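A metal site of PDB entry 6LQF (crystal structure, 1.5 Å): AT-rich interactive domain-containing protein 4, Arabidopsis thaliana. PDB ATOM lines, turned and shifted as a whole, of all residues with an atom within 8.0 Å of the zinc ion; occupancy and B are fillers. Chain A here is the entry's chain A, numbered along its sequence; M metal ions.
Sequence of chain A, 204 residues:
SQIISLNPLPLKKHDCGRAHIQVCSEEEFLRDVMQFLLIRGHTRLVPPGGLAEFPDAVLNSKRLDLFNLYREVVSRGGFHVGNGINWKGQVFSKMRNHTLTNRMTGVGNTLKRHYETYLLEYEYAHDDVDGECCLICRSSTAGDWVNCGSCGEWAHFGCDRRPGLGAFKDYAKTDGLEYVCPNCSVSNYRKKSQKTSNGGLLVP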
ATOM      1  N   LEU A 135      23.751  19.016   2.174  1.00  0.00           N
ATOM      2  CA  LEU A 135      23.413  19.526   3.500  1.00  0.00           C
ATOM      3  C   LEU A 135      22.332  20.570   3.390  1.00  0.00           C
ATOM      4  O   LEU A 135      21.657  20.842   4.393  1.00  0.00           O
ATOM      5  CB  LEU A 135      24.672  20.087   4.202  1.00  0.00           C
ATOM      6  CG  LEU A 135      25.383  21.287   3.541  1.00  0.00           C
ATOM      7  CD1 LEU A 135      24.864  22.627   4.045  1.00  0.00           C
ATOM      8  CD2 LEU A 135      26.901  21.224   3.758  1.00  0.00           C
ATOM      9  N   ASN A 147      32.768  20.409  -0.731  1.00  0.00           N
ATOM     10  CA  ASN A 147      32.816  19.890   0.624  1.00  0.00           C
ATOM     11  C   ASN A 147      33.108  21.072   1.580  1.00  0.00           C
ATOM     12  O   ASN A 147      34.053  21.859   1.342  1.00  0.00           O
ATOM     13  CB  ASN A 147      33.884  18.814   0.759  1.00  0.00           C
ATOM     14  CG  ASN A 147      33.893  18.190   2.161  1.00  0.00           C
ATOM     15  OD1 ASN A 147      34.827  18.399   2.938  1.00  0.00           O
ATOM     16  ND2 ASN A 147      32.883  17.433   2.472  1.00  0.00           N
ATOM     17  N   CYS A 148      32.316  21.204   2.629  1.00  0.00           N
ATOM     18  CA  CYS A 148      32.584  22.259   3.584  1.00  0.00           C
ATOM     19  C   CYS A 148      33.852  22.032   4.347  1.00  0.00           C
ATOM     20  O   CYS A 148      33.983  21.023   5.016  1.00  0.00           O
ATOM     21  CB  CYS A 148      31.399  22.371   4.516  1.00  0.00           C
ATOM     22  SG  CYS A 148      31.623  23.682   5.815  1.00  0.00           S
ATOM     23  N   GLY A 149      34.729  23.034   4.336  1.00  0.00           N
ATOM     24  CA  GLY A 149      35.997  22.931   5.068  1.00  0.00           C
ATOM     25  C   GLY A 149      35.802  22.965   6.588  1.00  0.00           C
ATOM     26  O   GLY A 149      36.711  22.586   7.340  1.00  0.00           O
ATOM     27  N   SER A 150      34.652  23.396   7.063  1.00  0.00           N
ATOM     28  CA  SER A 150      34.446  23.520   8.499  1.00  0.00           C
ATOM     29  C   SER A 150      33.791  22.256   9.096  1.00  0.00           C
ATOM     30  O   SER A 150      34.301  21.670  10.059  1.00  0.00           O
ATOM     31  CB  SER A 150      33.569  24.746   8.739  1.00  0.00           C
ATOM     32  OG  SER A 150      33.137  24.822  10.072  1.00  0.00           O
ATOM     33  N   CYS A 151      32.680  21.805   8.527  1.00  0.00           N
ATOM     34  CA  CYS A 151      31.951  20.681   9.097  1.00  0.00           C
ATOM     35  C   CYS A 151      32.190  19.367   8.352  1.00  0.00           C
ATOM     36  O   CYS A 151      31.776  18.326   8.856  1.00  0.00           O
ATOM     37  CB  CYS A 151      30.435  20.949   9.142  1.00  0.00           C
ATOM     38  SG  CYS A 151      29.591  21.093   7.541  1.00  0.00           S
ATOM     39  N   GLY A 152      32.767  19.437   7.152  1.00  0.00           N
ATOM     40  CA  GLY A 152      33.047  18.267   6.330  1.00  0.00           C
ATOM     41  C   GLY A 152      31.832  17.672   5.622  1.00  0.00           C
ATOM     42  O   GLY A 152      31.958  16.602   5.023  1.00  0.00           O
ATOM     43  N   GLU A 153      30.667  18.315   5.673  1.00  0.00           N
ATOM     44  CA  GLU A 153      29.525  17.830   4.928  1.00  0.00           C
ATOM     45  C   GLU A 153      29.602  18.334   3.492  1.00  0.00           C
ATOM     46  O   GLU A 153      30.420  19.207   3.157  1.00  0.00           O
ATOM     47  CB  GLU A 153      28.239  18.248   5.594  1.00  0.00           C
ATOM     48  CG  GLU A 153      28.066  17.559   6.912  1.00  0.00           C
ATOM     49  CD  GLU A 153      26.824  18.003   7.643  1.00  0.00           C
ATOM     50  OE1 GLU A 153      26.101  18.879   7.112  1.00  0.00           O
ATOM     51  OE2 GLU A 153      26.552  17.467   8.739  1.00  0.00           O
ATOM     52  N   TRP A 154      28.721  17.803   2.643  1.00  0.00           N
ATOM     53  CA  TRP A 154      28.752  18.130   1.239  1.00  0.00           C
ATOM     54  C   TRP A 154      27.528  18.915   0.787  1.00  0.00           C
ATOM     55  O   TRP A 154      26.471  18.699   1.316  1.00  0.00           O
ATOM     56  CB  TRP A 154      28.772  16.849   0.418  1.00  0.00           C
ATOM     57  CG  TRP A 154      30.114  16.115   0.403  1.00  0.00           C
ATOM     58  CD1 TRP A 154      30.521  15.104   1.216  1.00  0.00           C
ATOM     59  CD2 TRP A 154      31.157  16.330  -0.541  1.00  0.00           C
ATOM     60  NE1 TRP A 154      31.783  14.676   0.844  1.00  0.00           N
ATOM     61  CE2 TRP A 154      32.165  15.385  -0.269  1.00  0.00           C
ATOM     62  CE3 TRP A 154      31.286  17.179  -1.646  1.00  0.00           C
ATOM     63  CZ2 TRP A 154      33.354  15.338  -1.019  1.00  0.00           C
ATOM     64  CZ3 TRP A 154      32.452  17.136  -2.380  1.00  0.00           C
ATOM     65  CH2 TRP A 154      33.443  16.199  -2.121  1.00  0.00           C
ATOM     66  N   ALA A 155      27.748  19.877  -0.092  1.00  0.00           N
ATOM     67  CA  ALA A 155      26.660  20.704  -0.623  1.00  0.00           C
ATOM     68  C   ALA A 155      26.708  20.764  -2.138  1.00  0.00           C
ATOM     69  O   ALA A 155      27.774  20.855  -2.742  1.00  0.00           O
ATOM     70  CB  ALA A 155      26.741  22.108  -0.047  1.00  0.00           C
ATOM     71  N   TYR A 179      35.950  26.643   0.886  1.00  0.00           N
ATOM     72  CA  TYR A 179      34.505  26.696   0.928  1.00  0.00           C
ATOM     73  C   TYR A 179      34.008  26.455   2.364  1.00  0.00           C
ATOM     74  O   TYR A 179      34.374  25.474   2.981  1.00  0.00           O
ATOM     75  CB  TYR A 179      33.887  25.669  -0.016  1.00  0.00           C
ATOM     76  CG  TYR A 179      32.369  25.679   0.082  1.00  0.00           C
ATOM     77  CD1 TYR A 179      31.646  26.728  -0.446  1.00  0.00           C
ATOM     78  CD2 TYR A 179      31.680  24.648   0.730  1.00  0.00           C
ATOM     79  CE1 TYR A 179      30.265  26.764  -0.326  1.00  0.00           C
ATOM     80  CE2 TYR A 179      30.281  24.679   0.863  1.00  0.00           C
ATOM     81  CZ  TYR A 179      29.596  25.761   0.342  1.00  0.00           C
ATOM     82  OH  TYR A 179      28.208  25.851   0.439  1.00  0.00           O
ATOM     83  N   VAL A 180      33.143  27.348   2.864  1.00  0.00           N
ATOM     84  CA  VAL A 180      32.491  27.160   4.150  1.00  0.00           C
ATOM     85  C   VAL A 180      31.011  27.258   3.903  1.00  0.00           C
ATOM     86  O   VAL A 180      30.566  28.252   3.320  1.00  0.00           O
ATOM     87  CB  VAL A 180      32.963  28.211   5.178  1.00  0.00           C
ATOM     88  CG1 VAL A 180      32.182  28.116   6.469  1.00  0.00           C
ATOM     89  CG2 VAL A 180      34.463  28.020   5.440  1.00  0.00           C
ATOM     90  N   CYS A 181      30.263  26.260   4.318  1.00  0.00           N
ATOM     91  CA  CYS A 181      28.827  26.177   3.972  1.00  0.00           C
ATOM     92  C   CYS A 181      27.975  27.214   4.717  1.00  0.00           C
ATOM     93  O   CYS A 181      28.474  27.853   5.672  1.00  0.00           O
ATOM     94  CB  CYS A 181      28.317  24.733   4.283  1.00  0.00           C
ATOM     95  SG  CYS A 181      27.875  24.407   6.045  1.00  0.00           S
ATOM     96  N   PRO A 182      26.722  27.422   4.268  1.00  0.00           N
ATOM     97  CA  PRO A 182      25.898  28.472   4.904  1.00  0.00           C
ATOM     98  C   PRO A 182      25.610  28.163   6.363  1.00  0.00           C
ATOM     99  O   PRO A 182      25.438  29.090   7.154  1.00  0.00           O
ATOM    100  CB  PRO A 182      24.608  28.433   4.059  1.00  0.00           C
ATOM    101  CG  PRO A 182      25.006  27.888   2.727  1.00  0.00           C
ATOM    102  CD  PRO A 182      26.093  26.857   3.057  1.00  0.00           C
ATOM    103  N   ASN A 183      25.460  26.892   6.731  1.00  0.00           N
ATOM    104  CA  ASN A 183      25.191  26.559   8.127  1.00  0.00           C
ATOM    105  C   ASN A 183      26.367  26.837   9.069  1.00  0.00           C
ATOM    106  O   ASN A 183      26.146  27.199  10.228  1.00  0.00           O
ATOM    107  CB  ASN A 183      24.751  25.091   8.236  1.00  0.00           C
ATOM    108  CG  ASN A 183      23.432  24.857   7.524  1.00  0.00           C
ATOM    109  OD1 ASN A 183      22.750  25.829   7.156  1.00  0.00           O
ATOM    110  ND2 ASN A 183      23.038  23.614   7.361  1.00  0.00           N
ATOM    111  N   CYS A 184      27.604  26.698   8.587  1.00  0.00           N
ATOM    112  CA  CYS A 184      28.804  26.942   9.401  1.00  0.00           C
ATOM    113  C   CYS A 184      29.218  28.402   9.487  1.00  0.00           C
ATOM    114  O   CYS A 184      29.831  28.845  10.454  1.00  0.00           O
ATOM    115  CB  CYS A 184      29.987  26.166   8.820  1.00  0.00           C
ATOM    116  SG  CYS A 184      29.940  24.415   9.150  1.00  0.00           S
ATOM    117  N   SER A 185      28.915  29.159   8.447  1.00  0.00           N
ATOM    118  CA  SER A 185      29.420  30.517   8.308  1.00  0.00           C
ATOM    119  C   SER A 185      29.049  31.424   9.462  1.00  0.00           C
ATOM    120  O   SER A 185      27.890  31.480   9.865  1.00  0.00           O
ATOM    121  CB  SER A 185      28.910  31.117   7.006  1.00  0.00           C
ATOM    122  OG  SER A 185      29.673  30.583   5.925  1.00  0.00           O
HETATM  123 ZN    ZN M   1      29.688  23.427   7.104  1.00  0.00          ZN
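The side-chain sulfur of Cys 184 sits close to the side-chain hydroxyl of Ser 150 (3.4 Å).
N of Cys 148 sits at hydrogen-bond distance from O of Glu 153 (2.8 Å).
N of Asn 183 sits close to SG of Cys 181.
SG of Cys 151 lies close to N of Glu 153 (3.5 Å).
O of Cys 181 lies within hydrogen-bond range of OG of Ser 185 (3.0 Å).
The side-chain sulfur of Cys 148 sits close to the backbone NH of Ser 150 (3.3 Å).
Four residues have an atom within 4 Å of the zinc ion: Cys 148, Cys 151, Cys 181 and Cys 184.
Along chain A the residues within 4 Å of the zinc ion span positions 148 to 184.
The nearest printed residue that does not touch the zinc ion is Ser 150 (4.4 Å).
The zinc ion is bound by the side-chain sulfur (SG) of Cys 184, the side-chain sulfur (SG) of Cys 181, the side-chain sulfur (SG) of Cys 148 and the side-chain sulfur (SG) of Cys 151.
The zinc ion has four donor atoms within binding distance.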
